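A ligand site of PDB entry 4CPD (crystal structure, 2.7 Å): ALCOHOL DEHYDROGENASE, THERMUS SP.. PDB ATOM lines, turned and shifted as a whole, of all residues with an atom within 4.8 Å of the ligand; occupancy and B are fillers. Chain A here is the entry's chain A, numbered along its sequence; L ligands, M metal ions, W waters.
N of Pro 179 sits close to O9 of the ligand (3.2 Å). His 43 touches the ligand (CE1 to O13, 3.2 Å). CZ of Phe 85 touches O14 of the ligand (3.7 Å). OD1 of Asp 152 touches C20 of the ligand, 3.4 Å away. OG1 of Thr 156 touches C19 of the ligand, at 3.4 Å. CA of Gly 176 touches O4 of the ligand, at 3.9 Å. Gly 178 touches the ligand. Arg 201 touches the ligand. CD1 of Ile 202 touches O6 of the ligand (3.2 Å). Ala 243 touches the ligand. Gly 267 touches the ligand. Leu 292 touches the ligand. Phe 333 touches the ligand (CZ to O1, 3.3 Å). Hydrophobic or aromatic side chains within 4 Å of the ligand: His 43, Phe 85, Pro 179, Val 180, Ile 202, Val 244, Val 266, Val 268, Leu 292, Ala 293 and Phe 333. The nearest printed residue that does not touch the ligand is Ala 177 (4.1 Å).
The backbone NH (N) of Ala 293 lies within hydrogen-bond range of an oxygen (O14) of the ligand, at 2.7 Å. An oxygen (O1) of the ligand is in salt-bridge range of the guanidinium group of Arg 205 (3.5 Å). O of Val 266 sits at hydrogen-bond distance from N7 of the ligand (2.9 Å). O5 of the ligand is in hydrogen-bond range of OD2 of Asp 200, at 3.0 Å. The backbone carbonyl oxygen (O) of Val 244 lies within hydrogen-bond range of an oxygen (O12) of the ligand, at 3.0 Å. N of Val 268 sits at hydrogen-bond distance from O12 of the ligand, at 3.2 Å. N of Val 180 is in hydrogen-bond range of O9 of the ligand, 3.2 Å away. The backbone NH (N) of Gly 39 sits at hydrogen-bond distance from an oxygen (O8) of the ligand (3.2 Å). A nitrogen (N7) of the ligand is in hydrogen-bond range of the backbone carbonyl oxygen (O) of Gly 291 (3.3 Å). OG of Ser 40 is in hydrogen-bond range of O13 of the ligand.
OD1 of Asp 200 sits at hydrogen-bond distance from N of Ile 202 (3.4 Å). The side-chain carboxylate (OD2) of Asp 200 sits at hydrogen-bond distance from the backbone NH (N) of Ala 177 (2.6 Å). The backbone carbonyl oxygen (O) of Asp 200 sits at hydrogen-bond distance from the backbone NH (N) of Ala 219, 2.9 Å away. The side-chain sulfur of Cys 38 lies close to the backbone NH of Ser 40 (3.4 Å). The backbone carbonyl oxygen of Asp 152 is in hydrogen-bond range of the side-chain hydroxyl of Thr 156 (2.9 Å). The backbone carbonyl oxygen (O) of Ile 199 is in hydrogen-bond range of the backbone NH (N) of Gly 176 (2.8 Å).
Water W1 lies within hydrogen-bond range of an oxygen (O8) of the ligand (2.6 Å) and the backbone NH of Gly 39 (3.4 Å). Water W3 lies within hydrogen-bond range of O9 of the ligand, N of Gly 181, N of Gly 178 and O of Ala 243.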
ATOM      1  N   CYS A  38     -14.014   4.221 -25.748  1.00  0.00           N
ATOM      2  CA  CYS A  38     -12.665   4.395 -26.308  1.00  0.00           C
ATOM      3  C   CYS A  38     -11.621   4.060 -25.244  1.00  0.00           C
ATOM      4  O   CYS A  38     -11.883   4.129 -24.037  1.00  0.00           O
ATOM      5  CB  CYS A  38     -12.517   5.852 -26.804  1.00  0.00           C
ATOM      6  SG  CYS A  38     -10.919   6.306 -27.464  1.00  0.00           S
ATOM      7  N   GLY A  39     -10.429   3.711 -25.679  1.00  0.00           N
ATOM      8  CA  GLY A  39      -9.305   3.548 -24.773  1.00  0.00           C
ATOM      9  C   GLY A  39      -9.091   4.776 -23.895  1.00  0.00           C
ATOM     10  O   GLY A  39      -8.756   4.634 -22.717  1.00  0.00           O
ATOM     11  N   SER A  40      -9.289   5.973 -24.462  1.00  0.00           N
ATOM     12  CA  SER A  40      -9.197   7.225 -23.718  1.00  0.00           C
ATOM     13  C   SER A  40     -10.173   7.267 -22.543  1.00  0.00           C
ATOM     14  O   SER A  40      -9.897   7.895 -21.525  1.00  0.00           O
ATOM     15  CB  SER A  40      -9.470   8.439 -24.620  1.00  0.00           C
ATOM     16  OG  SER A  40      -8.574   8.476 -25.719  1.00  0.00           O
ATOM     17  N   LEU A  42     -10.894   4.856 -20.713  1.00  0.00           N
ATOM     18  CA  LEU A  42     -10.304   4.128 -19.586  1.00  0.00           C
ATOM     19  C   LEU A  42      -9.438   4.998 -18.683  1.00  0.00           C
ATOM     20  O   LEU A  42      -9.361   4.709 -17.509  1.00  0.00           O
ATOM     21  CB  LEU A  42      -9.514   2.926 -20.072  1.00  0.00           C
ATOM     22  CG  LEU A  42     -10.353   1.845 -20.739  1.00  0.00           C
ATOM     23  CD1 LEU A  42      -9.464   0.735 -21.283  1.00  0.00           C
ATOM     24  CD2 LEU A  42     -11.400   1.307 -19.756  1.00  0.00           C
ATOM     25  N   HIS A  43      -8.812   6.043 -19.225  1.00  0.00           N
ATOM     26  CA  HIS A  43      -8.060   6.993 -18.397  1.00  0.00           C
ATOM     27  C   HIS A  43      -9.009   7.762 -17.458  1.00  0.00           C
ATOM     28  O   HIS A  43      -8.679   8.016 -16.279  1.00  0.00           O
ATOM     29  CB  HIS A  43      -7.203   7.934 -19.238  1.00  0.00           C
ATOM     30  CG  HIS A  43      -6.301   7.208 -20.186  1.00  0.00           C
ATOM     31  ND1 HIS A  43      -6.230   7.500 -21.526  1.00  0.00           N
ATOM     32  CD2 HIS A  43      -5.453   6.177 -19.985  1.00  0.00           C
ATOM     33  CE1 HIS A  43      -5.353   6.697 -22.109  1.00  0.00           C
ATOM     34  NE2 HIS A  43      -4.879   5.875 -21.194  1.00  0.00           N
ATOM     35  N   PHE A  85     -14.164  13.814 -32.178  1.00  0.00           N
ATOM     36  CA  PHE A  85     -14.249  13.761 -30.754  1.00  0.00           C
ATOM     37  C   PHE A  85     -13.803  15.047 -30.056  1.00  0.00           C
ATOM     38  O   PHE A  85     -14.014  15.209 -28.874  1.00  0.00           O
ATOM     39  CB  PHE A  85     -13.441  12.586 -30.221  1.00  0.00           C
ATOM     40  CG  PHE A  85     -11.951  12.761 -30.308  1.00  0.00           C
ATOM     41  CD1 PHE A  85     -11.240  13.391 -29.287  1.00  0.00           C
ATOM     42  CD2 PHE A  85     -11.232  12.211 -31.358  1.00  0.00           C
ATOM     43  CE1 PHE A  85      -9.856  13.503 -29.331  1.00  0.00           C
ATOM     44  CE2 PHE A  85      -9.854  12.329 -31.413  1.00  0.00           C
ATOM     45  CZ  PHE A  85      -9.164  12.971 -30.399  1.00  0.00           C
ATOM     46  N   ASP A 152     -13.130   9.420 -34.531  1.00  0.00           N
ATOM     47  CA  ASP A 152     -12.066   9.271 -33.518  1.00  0.00           C
ATOM     48  C   ASP A 152     -10.981   8.311 -33.936  1.00  0.00           C
ATOM     49  O   ASP A 152     -10.019   8.730 -34.551  1.00  0.00           O
ATOM     50  CB  ASP A 152     -12.709   8.940 -32.158  1.00  0.00           C
ATOM     51  CG  ASP A 152     -11.730   8.754 -31.072  1.00  0.00           C
ATOM     52  OD1 ASP A 152     -10.502   8.796 -31.313  1.00  0.00           O
ATOM     53  OD2 ASP A 152     -12.193   8.527 -29.943  1.00  0.00           O
ATOM     54  N   ILE A 153     -11.110   7.026 -33.634  1.00  0.00           N
ATOM     55  CA  ILE A 153      -9.940   6.146 -33.723  1.00  0.00           C
ATOM     56  C   ILE A 153      -9.365   5.866 -35.150  1.00  0.00           C
ATOM     57  O   ILE A 153      -8.172   5.661 -35.302  1.00  0.00           O
ATOM     58  CB  ILE A 153     -10.151   4.830 -32.990  1.00  0.00           C
ATOM     59  CG1 ILE A 153     -11.339   4.074 -33.572  1.00  0.00           C
ATOM     60  CG2 ILE A 153     -10.375   5.063 -31.503  1.00  0.00           C
ATOM     61  CD1 ILE A 153     -11.288   2.610 -33.178  1.00  0.00           C
ATOM     62  N   THR A 156      -7.595   9.102 -36.241  1.00  0.00           N
ATOM     63  CA  THR A 156      -6.395   9.196 -35.428  1.00  0.00           C
ATOM     64  C   THR A 156      -5.252   8.402 -36.071  1.00  0.00           C
ATOM     65  O   THR A 156      -4.152   8.917 -36.256  1.00  0.00           O
ATOM     66  CB  THR A 156      -6.684   8.709 -33.984  1.00  0.00           C
ATOM     67  OG1 THR A 156      -7.562   9.631 -33.344  1.00  0.00           O
ATOM     68  CG2 THR A 156      -5.461   8.634 -33.167  1.00  0.00           C
ATOM     69  N   GLY A 176       1.260  -1.597 -30.610  1.00  0.00           N
ATOM     70  CA  GLY A 176      -0.079  -1.573 -30.048  1.00  0.00           C
ATOM     71  C   GLY A 176      -1.079  -2.082 -31.056  1.00  0.00           C
ATOM     72  O   GLY A 176      -1.322  -1.456 -32.079  1.00  0.00           O
ATOM     73  N   ALA A 177      -1.646  -3.247 -30.766  1.00  0.00           N
ATOM     74  CA  ALA A 177      -2.675  -3.856 -31.605  1.00  0.00           C
ATOM     75  C   ALA A 177      -4.083  -3.727 -30.998  1.00  0.00           C
ATOM     76  O   ALA A 177      -4.960  -4.507 -31.315  1.00  0.00           O
ATOM     77  CB  ALA A 177      -2.343  -5.317 -31.836  1.00  0.00           C
ATOM     78  N   GLY A 178      -4.289  -2.734 -30.135  1.00  0.00           N
ATOM     79  CA  GLY A 178      -5.642  -2.339 -29.755  1.00  0.00           C
ATOM     80  C   GLY A 178      -6.341  -1.649 -30.908  1.00  0.00           C
ATOM     81  O   GLY A 178      -5.784  -1.531 -32.024  1.00  0.00           O
ATOM     82  N   PRO A 179      -7.568  -1.170 -30.676  1.00  0.00           N
ATOM     83  CA  PRO A 179      -8.409  -0.567 -31.729  1.00  0.00           C
ATOM     84  C   PRO A 179      -7.674   0.415 -32.655  1.00  0.00           C
ATOM     85  O   PRO A 179      -7.835   0.359 -33.873  1.00  0.00           O
ATOM     86  CB  PRO A 179      -9.520   0.145 -30.948  1.00  0.00           C
ATOM     87  CG  PRO A 179      -9.644  -0.649 -29.684  1.00  0.00           C
ATOM     88  CD  PRO A 179      -8.286  -1.230 -29.384  1.00  0.00           C
ATOM     89  N   VAL A 180      -6.878   1.305 -32.068  1.00  0.00           N
ATOM     90  CA  VAL A 180      -6.183   2.325 -32.865  1.00  0.00           C
ATOM     91  C   VAL A 180      -5.141   1.680 -33.741  1.00  0.00           C
ATOM     92  O   VAL A 180      -5.106   1.947 -34.928  1.00  0.00           O
ATOM     93  CB  VAL A 180      -5.546   3.413 -31.977  1.00  0.00           C
ATOM     94  CG1 VAL A 180      -4.634   4.319 -32.782  1.00  0.00           C
ATOM     95  CG2 VAL A 180      -6.652   4.231 -31.296  1.00  0.00           C
ATOM     96  N   GLY A 181      -4.343   0.789 -33.148  1.00  0.00           N
ATOM     97  CA  GLY A 181      -3.359   0.025 -33.895  1.00  0.00           C
ATOM     98  C   GLY A 181      -3.950  -0.761 -35.049  1.00  0.00           C
ATOM     99  O   GLY A 181      -3.360  -0.861 -36.141  1.00  0.00           O
ATOM    100  N   ILE A 199       3.232  -5.122 -33.182  1.00  0.00           N
ATOM    101  CA  ILE A 199       3.842  -5.486 -31.936  1.00  0.00           C
ATOM    102  C   ILE A 199       2.803  -5.272 -30.861  1.00  0.00           C
ATOM    103  O   ILE A 199       2.255  -4.174 -30.741  1.00  0.00           O
ATOM    104  CB  ILE A 199       5.079  -4.621 -31.647  1.00  0.00           C
ATOM    105  CG1 ILE A 199       6.198  -4.931 -32.634  1.00  0.00           C
ATOM    106  CG2 ILE A 199       5.589  -4.860 -30.225  1.00  0.00           C
ATOM    107  CD1 ILE A 199       6.177  -4.099 -33.891  1.00  0.00           C
ATOM    108  N   ASP A 200       2.523  -6.326 -30.098  1.00  0.00           N
ATOM    109  CA  ASP A 200       1.669  -6.265 -28.917  1.00  0.00           C
ATOM    110  C   ASP A 200       2.052  -7.417 -27.984  1.00  0.00           C
ATOM    111  O   ASP A 200       3.088  -8.076 -28.208  1.00  0.00           O
ATOM    112  CB  ASP A 200       0.199  -6.356 -29.323  1.00  0.00           C
ATOM    113  CG  ASP A 200      -0.711  -5.729 -28.306  1.00  0.00           C
ATOM    114  OD1 ASP A 200      -0.664  -6.124 -27.130  1.00  0.00           O
ATOM    115  OD2 ASP A 200      -1.491  -4.829 -28.684  1.00  0.00           O
ATOM    116  N   ARG A 201       1.260  -7.646 -26.951  1.00  0.00           N
ATOM    117  CA  ARG A 201       1.504  -8.736 -26.028  1.00  0.00           C
ATOM    118  C   ARG A 201       0.232  -9.540 -25.676  1.00  0.00           C
ATOM    119  O   ARG A 201       0.148 -10.163 -24.612  1.00  0.00           O
ATOM    120  CB  ARG A 201       2.136  -8.176 -24.746  1.00  0.00           C
ATOM    121  CG  ARG A 201       1.196  -7.292 -23.944  1.00  0.00           C
ATOM    122  CD  ARG A 201       1.901  -6.616 -22.783  1.00  0.00           C
ATOM    123  NE  ARG A 201       0.944  -5.834 -22.004  1.00  0.00           N
ATOM    124  CZ  ARG A 201       1.287  -4.921 -21.094  1.00  0.00           C
ATOM    125  NH1 ARG A 201       2.566  -4.651 -20.842  1.00  0.00           N
ATOM    126  NH2 ARG A 201       0.340  -4.261 -20.447  1.00  0.00           N
ATOM    127  N   ILE A 202      -0.768  -9.525 -26.567  1.00  0.00           N
ATOM    128  CA  ILE A 202      -2.040 -10.242 -26.352  1.00  0.00           C
ATOM    129  C   ILE A 202      -2.428 -11.033 -27.599  1.00  0.00           C
ATOM    130  O   ILE A 202      -2.789 -10.435 -28.626  1.00  0.00           O
ATOM    131  CB  ILE A 202      -3.186  -9.283 -25.971  1.00  0.00           C
ATOM    132  CG1 ILE A 202      -2.868  -8.609 -24.625  1.00  0.00           C
ATOM    133  CG2 ILE A 202      -4.521 -10.024 -25.893  1.00  0.00           C
ATOM    134  CD1 ILE A 202      -3.916  -7.604 -24.174  1.00  0.00           C
ATOM    135  N   ARG A 205      -5.356 -10.188 -29.923  1.00  0.00           N
ATOM    136  CA  ARG A 205      -5.160  -8.940 -30.689  1.00  0.00           C
ATOM    137  C   ARG A 205      -4.149  -9.163 -31.818  1.00  0.00           C
ATOM    138  O   ARG A 205      -4.393  -8.755 -32.968  1.00  0.00           O
ATOM    139  CB  ARG A 205      -4.795  -7.763 -29.753  1.00  0.00           C
ATOM    140  CG  ARG A 205      -5.831  -7.588 -28.627  1.00  0.00           C
ATOM    141  CD  ARG A 205      -5.847  -6.247 -27.897  1.00  0.00           C
ATOM    142  NE  ARG A 205      -7.188  -5.920 -27.355  1.00  0.00           N
ATOM    143  CZ  ARG A 205      -7.501  -4.801 -26.707  1.00  0.00           C
ATOM    144  NH1 ARG A 205      -6.572  -3.869 -26.493  1.00  0.00           N
ATOM    145  NH2 ARG A 205      -8.740  -4.589 -26.259  1.00  0.00           N
ATOM    146  N   ALA A 219       5.830  -9.102 -27.956  1.00  0.00           N
ATOM    147  CA  ALA A 219       6.949  -8.449 -27.257  1.00  0.00           C
ATOM    148  C   ALA A 219       7.321  -9.099 -25.923  1.00  0.00           C
ATOM    149  O   ALA A 219       8.423  -8.873 -25.413  1.00  0.00           O
ATOM    150  CB  ALA A 219       6.645  -6.973 -27.027  1.00  0.00           C
ATOM    151  N   ALA A 243       1.262   3.387 -30.734  1.00  0.00           N
ATOM    152  CA  ALA A 243      -0.142   3.560 -30.372  1.00  0.00           C
ATOM    153  C   ALA A 243      -0.459   2.969 -29.012  1.00  0.00           C
ATOM    154  O   ALA A 243      -1.597   2.519 -28.780  1.00  0.00           O
ATOM    155  CB  ALA A 243      -1.039   2.930 -31.420  1.00  0.00           C
ATOM    156  N   VAL A 244       0.536   2.942 -28.117  1.00  0.00           N
ATOM    157  CA  VAL A 244       0.312   2.454 -26.785  1.00  0.00           C
ATOM    158  C   VAL A 244       0.297   3.607 -25.798  1.00  0.00           C
ATOM    159  O   VAL A 244      -0.682   3.770 -25.065  1.00  0.00           O
ATOM    160  CB  VAL A 244       1.405   1.447 -26.399  1.00  0.00           C
ATOM    161  CG1 VAL A 244       1.234   1.034 -24.950  1.00  0.00           C
ATOM    162  CG2 VAL A 244       1.326   0.230 -27.314  1.00  0.00           C
ATOM    163  N   GLY A 245       1.388   4.365 -25.785  1.00  0.00           N
ATOM    164  CA  GLY A 245       1.608   5.458 -24.812  1.00  0.00           C
ATOM    165  C   GLY A 245       2.706   5.074 -23.825  1.00  0.00           C
ATOM    166  O   GLY A 245       2.695   3.967 -23.289  1.00  0.00           O
ATOM    167  N   THR A 249       7.507   2.127 -24.837  1.00  0.00           N
ATOM    168  CA  THR A 249       7.182   1.941 -26.257  1.00  0.00           C
ATOM    169  C   THR A 249       7.757   3.044 -27.170  1.00  0.00           C
ATOM    170  O   THR A 249       8.051   2.791 -28.341  1.00  0.00           O
ATOM    171  CB  THR A 249       5.664   1.835 -26.466  1.00  0.00           C
ATOM    172  OG1 THR A 249       4.978   2.868 -25.733  1.00  0.00           O
ATOM    173  CG2 THR A 249       5.182   0.496 -25.986  1.00  0.00           C
ATOM    174  N   VAL A 266       1.307   8.436 -31.098  1.00  0.00           N
ATOM    175  CA  VAL A 266      -0.102   8.744 -31.043  1.00  0.00           C
ATOM    176  C   VAL A 266      -0.737   8.255 -29.711  1.00  0.00           C
ATOM    177  O   VAL A 266      -1.807   8.696 -29.330  1.00  0.00           O
ATOM    178  CB  VAL A 266      -0.776   8.163 -32.309  1.00  0.00           C
ATOM    179  CG1 VAL A 266      -1.624   6.961 -31.937  1.00  0.00           C
ATOM    180  CG2 VAL A 266      -1.612   9.192 -33.011  1.00  0.00           C
ATOM    181  N   GLY A 267      -0.037   7.394 -28.994  1.00  0.00           N
ATOM    182  CA  GLY A 267      -0.473   6.954 -27.661  1.00  0.00           C
ATOM    183  C   GLY A 267      -0.359   7.987 -26.519  1.00  0.00           C
ATOM    184  O   GLY A 267       0.629   8.725 -26.401  1.00  0.00           O
ATOM    185  N   VAL A 268      -1.373   7.987 -25.653  1.00  0.00           N
ATOM    186  CA  VAL A 268      -1.436   8.882 -24.506  1.00  0.00           C
ATOM    187  C   VAL A 268      -0.782   8.293 -23.249  1.00  0.00           C
ATOM    188  O   VAL A 268      -0.875   7.086 -23.029  1.00  0.00           O
ATOM    189  CB  VAL A 268      -2.911   9.249 -24.205  1.00  0.00           C
ATOM    190  CG1 VAL A 268      -3.045  10.075 -22.928  1.00  0.00           C
ATOM    191  CG2 VAL A 268      -3.506  10.026 -25.374  1.00  0.00           C
ATOM    192  N   GLY A 291       1.438  13.934 -30.649  1.00  0.00           N
ATOM    193  CA  GLY A 291       0.297  14.821 -30.537  1.00  0.00           C
ATOM    194  C   GLY A 291      -1.054  14.150 -30.472  1.00  0.00           C
ATOM    195  O   GLY A 291      -1.192  12.950 -30.708  1.00  0.00           O
ATOM    196  N   LEU A 292      -2.064  14.945 -30.160  1.00  0.00           N
ATOM    197  CA  LEU A 292      -3.434  14.499 -30.230  1.00  0.00           C
ATOM    198  C   LEU A 292      -3.946  14.714 -31.656  1.00  0.00           C
ATOM    199  O   LEU A 292      -3.525  15.644 -32.361  1.00  0.00           O
ATOM    200  CB  LEU A 292      -4.275  15.286 -29.228  1.00  0.00           C
ATOM    201  CG  LEU A 292      -3.750  15.296 -27.785  1.00  0.00           C
ATOM    202  CD1 LEU A 292      -4.748  15.980 -26.866  1.00  0.00           C
ATOM    203  CD2 LEU A 292      -3.459  13.895 -27.235  1.00  0.00           C
ATOM    204  N   ALA A 293      -4.873  13.863 -32.070  1.00  0.00           N
ATOM    205  CA  ALA A 293      -5.332  13.838 -33.452  1.00  0.00           C
ATOM    206  C   ALA A 293      -5.899  15.128 -33.883  1.00  0.00           C
ATOM    207  O   ALA A 293      -6.454  15.852 -33.077  1.00  0.00           O
ATOM    208  CB  ALA A 293      -6.396  12.795 -33.604  1.00  0.00           C
ATOM    209  N   PHE A 333     -14.260  -4.054 -21.508  1.00  0.00           N
ATOM    210  CA  PHE A 333     -13.189  -3.374 -22.245  1.00  0.00           C
ATOM    211  C   PHE A 333     -11.946  -3.160 -21.377  1.00  0.00           C
ATOM    212  O   PHE A 333     -10.821  -3.429 -21.793  1.00  0.00           O
ATOM    213  CB  PHE A 333     -13.708  -2.050 -22.814  1.00  0.00           C
ATOM    214  CG  PHE A 333     -12.739  -1.376 -23.736  1.00  0.00           C
ATOM    215  CD1 PHE A 333     -12.153  -2.087 -24.786  1.00  0.00           C
ATOM    216  CD2 PHE A 333     -12.425  -0.035 -23.569  1.00  0.00           C
ATOM    217  CE1 PHE A 333     -11.261  -1.448 -25.648  1.00  0.00           C
ATOM    218  CE2 PHE A 333     -11.551   0.596 -24.424  1.00  0.00           C
ATOM    219  CZ  PHE A 333     -10.963  -0.113 -25.465  1.00  0.00           C
HETATM  220  P1  LIG L   1      -6.343   0.084 -25.695  1.00  0.00           P
HETATM  221  O1  LIG L   1      -7.679  -0.618 -25.881  1.00  0.00           O
HETATM  222  O2  LIG L   1      -5.789   0.276 -24.283  1.00  0.00           O
HETATM  223  O3  LIG L   1      -5.157  -0.556 -26.588  1.00  0.00           O
HETATM  224  C1  LIG L   1      -3.809  -0.601 -26.119  1.00  0.00           C
HETATM  225  C2  LIG L   1      -3.096  -1.818 -26.676  1.00  0.00           C
HETATM  226  O4  LIG L   1      -1.680  -1.696 -26.466  1.00  0.00           O
HETATM  227  C3  LIG L   1      -3.563  -3.103 -25.990  1.00  0.00           C
HETATM  228  O5  LIG L   1      -3.785  -4.191 -26.900  1.00  0.00           O
HETATM  229  C4  LIG L   1      -2.403  -3.463 -25.088  1.00  0.00           C
HETATM  230  O6  LIG L   1      -2.315  -4.870 -24.866  1.00  0.00           O
HETATM  231  C5  LIG L   1      -1.243  -2.913 -25.881  1.00  0.00           C
HETATM  232  N1  LIG L   1      -0.090  -2.688 -24.991  1.00  0.00           N
HETATM  233  C6  LIG L   1      -0.162  -2.131 -23.771  1.00  0.00           C
HETATM  234  N2  LIG L   1       1.086  -2.086 -23.234  1.00  0.00           N
HETATM  235  C7  LIG L   1       1.944  -2.625 -24.120  1.00  0.00           C
HETATM  236  C8  LIG L   1       3.401  -2.875 -24.191  1.00  0.00           C
HETATM  237  N3  LIG L   1       4.165  -2.509 -23.151  1.00  0.00           N
HETATM  238  N4  LIG L   1       3.929  -3.464 -25.299  1.00  0.00           N
HETATM  239  C9  LIG L   1       3.155  -3.812 -26.341  1.00  0.00           C
HETATM  240  N5  LIG L   1       1.813  -3.611 -26.341  1.00  0.00           N
HETATM  241  C10 LIG L   1       1.163  -3.036 -25.294  1.00  0.00           C
HETATM  242  O7  LIG L   1      -6.418   1.577 -26.334  1.00  0.00           O
HETATM  243  P2  LIG L   1      -6.887   2.024 -27.817  1.00  0.00           P
HETATM  244  O8  LIG L   1      -8.383   2.212 -27.710  1.00  0.00           O
HETATM  245  O9  LIG L   1      -6.208   1.188 -28.903  1.00  0.00           O
HETATM  246  O10 LIG L   1      -6.160   3.464 -27.918  1.00  0.00           O
HETATM  247  C11 LIG L   1      -4.753   3.477 -28.252  1.00  0.00           C
HETATM  248  C12 LIG L   1      -3.933   4.580 -27.606  1.00  0.00           C
HETATM  249  O11 LIG L   1      -4.057   5.758 -28.410  1.00  0.00           O
HETATM  250  C13 LIG L   1      -4.375   4.962 -26.195  1.00  0.00           C
HETATM  251  O12 LIG L   1      -3.222   5.366 -25.444  1.00  0.00           O
HETATM  252  C14 LIG L   1      -5.360   6.111 -26.420  1.00  0.00           C
HETATM  253  O13 LIG L   1      -5.586   6.986 -25.291  1.00  0.00           O
HETATM  254  C15 LIG L   1      -4.684   6.795 -27.609  1.00  0.00           C
HETATM  255  N6  LIG L   1      -5.583   7.632 -28.417  1.00  0.00           N
HETATM  256  C16 LIG L   1      -5.043   8.794 -28.816  1.00  0.00           C
HETATM  257  C17 LIG L   1      -5.740   9.708 -29.579  1.00  0.00           C
HETATM  258  C18 LIG L   1      -5.001  10.954 -29.965  1.00  0.00           C
HETATM  259  O14 LIG L   1      -5.596  12.001 -30.192  1.00  0.00           O
HETATM  260  N7  LIG L   1      -3.661  10.865 -30.077  1.00  0.00           N
HETATM  261  C19 LIG L   1      -7.066   9.412 -29.961  1.00  0.00           C
HETATM  262  C20 LIG L   1      -7.621   8.198 -29.546  1.00  0.00           C
HETATM  263  C21 LIG L   1      -6.859   7.309 -28.763  1.00  0.00           C
HETATM  264 ZN    ZN M   1     -11.323   8.373 -28.231  1.00  0.00          ZN
HETATM  265  O   HOH W   1     -10.745   2.586 -28.825  1.00  0.00           O
HETATM  266  O   HOH W   2      -9.426   9.958 -28.064  1.00  0.00           O
HETATM  267  O   HOH W   3      -3.680   0.431 -30.188  1.00  0.00           O
